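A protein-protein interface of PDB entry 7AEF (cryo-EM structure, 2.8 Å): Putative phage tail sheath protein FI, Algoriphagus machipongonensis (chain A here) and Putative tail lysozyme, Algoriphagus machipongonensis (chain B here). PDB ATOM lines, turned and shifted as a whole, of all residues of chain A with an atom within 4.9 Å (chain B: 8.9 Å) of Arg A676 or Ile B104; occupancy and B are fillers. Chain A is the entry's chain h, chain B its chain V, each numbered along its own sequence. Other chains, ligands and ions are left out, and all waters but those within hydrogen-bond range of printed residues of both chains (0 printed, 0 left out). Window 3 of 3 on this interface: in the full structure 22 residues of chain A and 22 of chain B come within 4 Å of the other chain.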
ATOM      1  N   ASN A 582     -20.126  31.132  28.536  1.00  0.00           N
ATOM      2  CA  ASN A 582     -18.772  30.855  28.090  1.00  0.00           C
ATOM      3  C   ASN A 582     -17.903  30.160  29.130  1.00  0.00           C
ATOM      4  O   ASN A 582     -16.933  29.499  28.757  1.00  0.00           O
ATOM      5  CB  ASN A 582     -18.127  32.136  27.629  1.00  0.00           C
ATOM      6  CG  ASN A 582     -18.684  32.583  26.315  1.00  0.00           C
ATOM      7  OD1 ASN A 582     -19.174  31.778  25.519  1.00  0.00           O
ATOM      8  ND2 ASN A 582     -18.638  33.863  26.077  1.00  0.00           N
ATOM      9  N   GLU A 583     -18.194  30.302  30.421  1.00  0.00           N
ATOM     10  CA  GLU A 583     -17.350  29.667  31.425  1.00  0.00           C
ATOM     11  C   GLU A 583     -18.008  28.486  32.113  1.00  0.00           C
ATOM     12  O   GLU A 583     -17.350  27.465  32.338  1.00  0.00           O
ATOM     13  CB  GLU A 583     -16.946  30.684  32.493  1.00  0.00           C
ATOM     14  CG  GLU A 583     -16.098  31.837  31.990  1.00  0.00           C
ATOM     15  CD  GLU A 583     -15.728  32.827  33.072  1.00  0.00           C
ATOM     16  OE1 GLU A 583     -16.156  32.662  34.198  1.00  0.00           O
ATOM     17  OE2 GLU A 583     -15.009  33.764  32.780  1.00  0.00           O
ATOM     18  N   ARG A 585     -20.910  26.430  31.247  1.00  0.00           N
ATOM     19  CA  ARG A 585     -21.880  25.561  30.575  1.00  0.00           C
ATOM     20  C   ARG A 585     -21.719  24.071  30.864  1.00  0.00           C
ATOM     21  O   ARG A 585     -22.685  23.322  30.706  1.00  0.00           O
ATOM     22  CB  ARG A 585     -21.863  25.750  29.065  1.00  0.00           C
ATOM     23  CG  ARG A 585     -20.654  25.269  28.346  1.00  0.00           C
ATOM     24  CD  ARG A 585     -20.777  25.512  26.895  1.00  0.00           C
ATOM     25  NE  ARG A 585     -20.765  26.929  26.588  1.00  0.00           N
ATOM     26  CZ  ARG A 585     -20.953  27.462  25.384  1.00  0.00           C
ATOM     27  NH1 ARG A 585     -21.156  26.704  24.329  1.00  0.00           N
ATOM     28  NH2 ARG A 585     -20.928  28.771  25.265  1.00  0.00           N
ATOM     29  N   TYR A 586     -20.542  23.612  31.271  1.00  0.00           N
ATOM     30  CA  TYR A 586     -20.361  22.187  31.505  1.00  0.00           C
ATOM     31  C   TYR A 586     -20.445  21.840  32.972  1.00  0.00           C
ATOM     32  O   TYR A 586     -19.929  22.568  33.824  1.00  0.00           O
ATOM     33  CB  TYR A 586     -19.032  21.693  30.963  1.00  0.00           C
ATOM     34  CG  TYR A 586     -18.942  21.761  29.487  1.00  0.00           C
ATOM     35  CD1 TYR A 586     -18.095  22.658  28.891  1.00  0.00           C
ATOM     36  CD2 TYR A 586     -19.729  20.943  28.702  1.00  0.00           C
ATOM     37  CE1 TYR A 586     -18.020  22.733  27.540  1.00  0.00           C
ATOM     38  CE2 TYR A 586     -19.664  21.016  27.348  1.00  0.00           C
ATOM     39  CZ  TYR A 586     -18.808  21.908  26.763  1.00  0.00           C
ATOM     40  OH  TYR A 586     -18.719  22.005  25.395  1.00  0.00           O
ATOM     41  N   VAL A 589     -16.942  21.224  34.667  1.00  0.00           N
ATOM     42  CA  VAL A 589     -16.151  22.399  34.968  1.00  0.00           C
ATOM     43  C   VAL A 589     -16.601  23.000  36.280  1.00  0.00           C
ATOM     44  O   VAL A 589     -15.775  23.309  37.135  1.00  0.00           O
ATOM     45  CB  VAL A 589     -16.210  23.419  33.828  1.00  0.00           C
ATOM     46  CG1 VAL A 589     -15.516  24.719  34.244  1.00  0.00           C
ATOM     47  CG2 VAL A 589     -15.527  22.821  32.596  1.00  0.00           C
ATOM     48  N   VAL A 674      -8.592  25.374  32.646  1.00  0.00           N
ATOM     49  CA  VAL A 674      -9.116  24.026  32.865  1.00  0.00           C
ATOM     50  C   VAL A 674      -9.423  23.316  31.555  1.00  0.00           C
ATOM     51  O   VAL A 674      -9.670  23.936  30.519  1.00  0.00           O
ATOM     52  CB  VAL A 674     -10.408  24.081  33.694  1.00  0.00           C
ATOM     53  CG1 VAL A 674     -10.109  24.646  35.093  1.00  0.00           C
ATOM     54  CG2 VAL A 674     -11.494  24.868  32.979  1.00  0.00           C
ATOM     55  N   VAL A 675      -9.481  21.999  31.650  1.00  0.00           N
ATOM     56  CA  VAL A 675      -9.775  21.110  30.533  1.00  0.00           C
ATOM     57  C   VAL A 675     -11.276  21.008  30.263  1.00  0.00           C
ATOM     58  O   VAL A 675     -12.067  20.816  31.188  1.00  0.00           O
ATOM     59  CB  VAL A 675      -9.178  19.732  30.831  1.00  0.00           C
ATOM     60  CG1 VAL A 675      -9.547  18.728  29.756  1.00  0.00           C
ATOM     61  CG2 VAL A 675      -7.660  19.875  30.954  1.00  0.00           C
ATOM     62  N   ARG A 676     -11.669  21.123  28.990  1.00  0.00           N
ATOM     63  CA  ARG A 676     -13.058  21.018  28.569  1.00  0.00           C
ATOM     64  C   ARG A 676     -13.214  19.813  27.614  1.00  0.00           C
ATOM     65  O   ARG A 676     -12.250  19.460  26.944  1.00  0.00           O
ATOM     66  CB  ARG A 676     -13.462  22.353  27.935  1.00  0.00           C
ATOM     67  CG  ARG A 676     -13.422  23.474  28.961  1.00  0.00           C
ATOM     68  CD  ARG A 676     -13.688  24.802  28.422  1.00  0.00           C
ATOM     69  NE  ARG A 676     -13.526  25.813  29.475  1.00  0.00           N
ATOM     70  CZ  ARG A 676     -14.502  26.269  30.286  1.00  0.00           C
ATOM     71  NH1 ARG A 676     -15.739  25.856  30.188  1.00  0.00           N
ATOM     72  NH2 ARG A 676     -14.254  27.163  31.215  1.00  0.00           N
ATOM     73  N   PRO A 677     -14.391  19.152  27.591  1.00  0.00           N
ATOM     74  CA  PRO A 677     -14.690  17.950  26.786  1.00  0.00           C
ATOM     75  C   PRO A 677     -14.943  18.180  25.303  1.00  0.00           C
ATOM     76  O   PRO A 677     -15.368  19.250  24.886  1.00  0.00           O
ATOM     77  CB  PRO A 677     -15.996  17.470  27.421  1.00  0.00           C
ATOM     78  CG  PRO A 677     -16.638  18.722  27.926  1.00  0.00           C
ATOM     79  CD  PRO A 677     -15.520  19.573  28.417  1.00  0.00           C
ATOM     80  N   ALA A 678     -14.750  17.128  24.509  1.00  0.00           N
ATOM     81  CA  ALA A 678     -15.163  17.170  23.114  1.00  0.00           C
ATOM     82  C   ALA A 678     -16.596  16.679  22.975  1.00  0.00           C
ATOM     83  O   ALA A 678     -16.936  15.621  23.501  1.00  0.00           O
ATOM     84  CB  ALA A 678     -14.251  16.311  22.260  1.00  0.00           C
ATOM     85  N   PHE B  65     -17.422  12.859  24.649  1.00  0.00           N
ATOM     86  CA  PHE B  65     -17.346  13.318  26.043  1.00  0.00           C
ATOM     87  C   PHE B  65     -16.064  12.865  26.734  1.00  0.00           C
ATOM     88  O   PHE B  65     -16.084  12.450  27.892  1.00  0.00           O
ATOM     89  CB  PHE B  65     -18.554  12.868  26.874  1.00  0.00           C
ATOM     90  CG  PHE B  65     -19.848  13.309  26.329  1.00  0.00           C
ATOM     91  CD1 PHE B  65     -20.634  12.453  25.585  1.00  0.00           C
ATOM     92  CD2 PHE B  65     -20.295  14.581  26.573  1.00  0.00           C
ATOM     93  CE1 PHE B  65     -21.839  12.870  25.092  1.00  0.00           C
ATOM     94  CE2 PHE B  65     -21.496  15.003  26.085  1.00  0.00           C
ATOM     95  CZ  PHE B  65     -22.270  14.147  25.345  1.00  0.00           C
ATOM     96  N   SER B  66     -14.940  12.979  26.042  1.00  0.00           N
ATOM     97  CA  SER B  66     -13.651  12.595  26.580  1.00  0.00           C
ATOM     98  C   SER B  66     -12.646  13.690  26.238  1.00  0.00           C
ATOM     99  O   SER B  66     -12.856  14.434  25.276  1.00  0.00           O
ATOM    100  CB  SER B  66     -13.209  11.249  25.990  1.00  0.00           C
ATOM    101  OG  SER B  66     -12.934  11.395  24.616  1.00  0.00           O
ATOM    102  N   PRO B  67     -11.588  13.843  27.047  1.00  0.00           N
ATOM    103  CA  PRO B  67     -10.496  14.794  26.768  1.00  0.00           C
ATOM    104  C   PRO B  67      -9.624  14.308  25.628  1.00  0.00           C
ATOM    105  O   PRO B  67      -9.535  13.113  25.363  1.00  0.00           O
ATOM    106  CB  PRO B  67      -9.708  14.796  28.085  1.00  0.00           C
ATOM    107  CG  PRO B  67     -10.008  13.450  28.691  1.00  0.00           C
ATOM    108  CD  PRO B  67     -11.413  13.158  28.333  1.00  0.00           C
ATOM    109  N   ILE B  68      -8.935  15.245  24.983  1.00  0.00           N
ATOM    110  CA  ILE B  68      -8.101  14.941  23.827  1.00  0.00           C
ATOM    111  C   ILE B  68      -6.628  14.871  24.225  1.00  0.00           C
ATOM    112  O   ILE B  68      -6.072  15.843  24.744  1.00  0.00           O
ATOM    113  CB  ILE B  68      -8.312  15.961  22.702  1.00  0.00           C
ATOM    114  CG1 ILE B  68      -9.782  15.967  22.273  1.00  0.00           C
ATOM    115  CG2 ILE B  68      -7.417  15.663  21.516  1.00  0.00           C
ATOM    116  CD1 ILE B  68     -10.242  17.232  21.576  1.00  0.00           C
ATOM    117  N   GLN B 100      -7.542  19.760  17.045  1.00  0.00           N
ATOM    118  CA  GLN B 100      -8.593  20.453  17.795  1.00  0.00           C
ATOM    119  C   GLN B 100      -8.631  21.924  17.387  1.00  0.00           C
ATOM    120  O   GLN B 100      -7.701  22.674  17.682  1.00  0.00           O
ATOM    121  CB  GLN B 100      -8.346  20.312  19.296  1.00  0.00           C
ATOM    122  CG  GLN B 100      -9.380  20.982  20.146  1.00  0.00           C
ATOM    123  CD  GLN B 100      -9.125  20.804  21.618  1.00  0.00           C
ATOM    124  OE1 GLN B 100      -8.314  19.972  22.030  1.00  0.00           O
ATOM    125  NE2 GLN B 100      -9.766  21.638  22.427  1.00  0.00           N
ATOM    126  N   GLY B 101      -9.706  22.344  16.724  1.00  0.00           N
ATOM    127  CA  GLY B 101      -9.801  23.700  16.211  1.00  0.00           C
ATOM    128  C   GLY B 101     -10.530  24.689  17.098  1.00  0.00           C
ATOM    129  O   GLY B 101     -10.710  25.852  16.698  1.00  0.00           O
ATOM    130  N   ASN B 102     -10.949  24.269  18.301  1.00  0.00           N
ATOM    131  CA  ASN B 102     -11.770  25.112  19.170  1.00  0.00           C
ATOM    132  C   ASN B 102     -11.353  24.923  20.629  1.00  0.00           C
ATOM    133  O   ASN B 102     -11.418  23.815  21.178  1.00  0.00           O
ATOM    134  CB  ASN B 102     -13.211  24.687  18.996  1.00  0.00           C
ATOM    135  CG  ASN B 102     -13.913  25.408  17.883  1.00  0.00           C
ATOM    136  OD1 ASN B 102     -14.239  26.580  17.928  1.00  0.00           O
ATOM    137  ND2 ASN B 102     -13.974  24.695  16.759  1.00  0.00           N
ATOM    138  N   GLU B 103     -10.989  26.032  21.260  1.00  0.00           N
ATOM    139  CA  GLU B 103     -10.625  26.089  22.676  1.00  0.00           C
ATOM    140  C   GLU B 103     -11.815  25.760  23.560  1.00  0.00           C
ATOM    141  O   GLU B 103     -11.657  25.136  24.617  1.00  0.00           O
ATOM    142  CB  GLU B 103     -10.130  27.511  22.952  1.00  0.00           C
ATOM    143  CG  GLU B 103      -8.811  27.801  22.258  1.00  0.00           C
ATOM    144  CD  GLU B 103      -9.048  28.365  20.863  1.00  0.00           C
ATOM    145  OE1 GLU B 103     -10.211  28.376  20.421  1.00  0.00           O
ATOM    146  OE2 GLU B 103      -8.080  28.648  20.157  1.00  0.00           O
ATOM    147  N   ILE B 104     -13.013  26.193  23.158  1.00  0.00           N
ATOM    148  CA  ILE B 104     -14.220  26.035  23.964  1.00  0.00           C
ATOM    149  C   ILE B 104     -15.187  25.016  23.372  1.00  0.00           C
ATOM    150  O   ILE B 104     -15.641  24.115  24.079  1.00  0.00           O
ATOM    151  CB  ILE B 104     -14.925  27.385  24.197  1.00  0.00           C
ATOM    152  CG1 ILE B 104     -13.971  28.392  24.863  1.00  0.00           C
ATOM    153  CG2 ILE B 104     -16.209  27.163  25.007  1.00  0.00           C
ATOM    154  CD1 ILE B 104     -13.412  27.993  26.236  1.00  0.00           C
ATOM    155  N   GLU B 105     -15.589  25.196  22.108  1.00  0.00           N
ATOM    156  CA  GLU B 105     -16.555  24.269  21.523  1.00  0.00           C
ATOM    157  C   GLU B 105     -15.995  22.851  21.524  1.00  0.00           C
ATOM    158  O   GLU B 105     -14.805  22.642  21.296  1.00  0.00           O
ATOM    159  CB  GLU B 105     -16.920  24.695  20.100  1.00  0.00           C
ATOM    160  CG  GLU B 105     -17.703  25.997  20.024  1.00  0.00           C
ATOM    161  CD  GLU B 105     -17.984  26.423  18.595  1.00  0.00           C
ATOM    162  OE1 GLU B 105     -17.412  25.813  17.668  1.00  0.00           O
ATOM    163  OE2 GLU B 105     -18.775  27.370  18.400  1.00  0.00           O
ATOM    164  N   GLY B 106     -16.845  21.881  21.838  1.00  0.00           N
ATOM    165  CA  GLY B 106     -16.397  20.502  21.914  1.00  0.00           C
ATOM    166  C   GLY B 106     -16.176  19.852  20.565  1.00  0.00           C
ATOM    167  O   GLY B 106     -16.888  18.915  20.196  1.00  0.00           O
ATOM    168  N   GLU B 107     -15.184  20.317  19.814  1.00  0.00           N
ATOM    169  CA  GLU B 107     -14.956  19.815  18.469  1.00  0.00           C
ATOM    170  C   GLU B 107     -13.602  19.136  18.300  1.00  0.00           C
ATOM    171  O   GLU B 107     -12.568  19.647  18.735  1.00  0.00           O
ATOM    172  CB  GLU B 107     -15.065  20.923  17.447  1.00  0.00           C
ATOM    173  CG  GLU B 107     -16.436  21.522  17.325  1.00  0.00           C
ATOM    174  CD  GLU B 107     -16.499  22.521  16.213  1.00  0.00           C
ATOM    175  OE1 GLU B 107     -15.456  22.781  15.608  1.00  0.00           O
ATOM    176  OE2 GLU B 107     -17.578  23.050  15.935  1.00  0.00           O
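Printed residues of chain A that touch a printed residue of chain B: Tyr A586, Arg A676, Pro A677 and Ala A678.
Along chain A the printed residues that touch a printed residue of chain B span positions 586 to 678.
Among the printed residues, 6 pairs touch across the chains.
O of Ser B66 is in hydrogen-bond range of N of Ala A678 (3.4 Å).
O of Ala A678 lies within hydrogen-bond range of N of Phe B65 (3.0 Å).
Of the printed residues of chain B, Arg A676 touches Ile B104 (3.9 Å).
Ile B104 touches just these residues of chain A: Tyr A586 (3.96 Å) and Arg A676 (3.9 Å).
No residue of chain B comes within 4 Å of Val A675.
Of the printed residues of chain A, Gly B106 touches Pro A677 (3.4 Å) and Ala A678 (3.6 Å).
Of the printed residues of chain A, Ser B66 touches Ala A678 (3.4 Å).
Glu A583 touches none of the printed residues of chain B.
The nearest residue of chain A that does not touch Ile B104 is Asn A582 (4.5 Å).
The nearest printed residue of chain A that does not touch Ser B66 is Pro A677 (4.2 Å).
Tyr A586 touches Ile B104.
Arg A676 touches Ile B104 (CD to CD1, 3.9 Å).
O of Pro A677 touches CA of Gly B106, at 3.4 Å.
Ala A678 touches Gly B106.
NH1 of Arg A676 is in hydrogen-bond range of O of Glu A583, 3.1 Å away.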
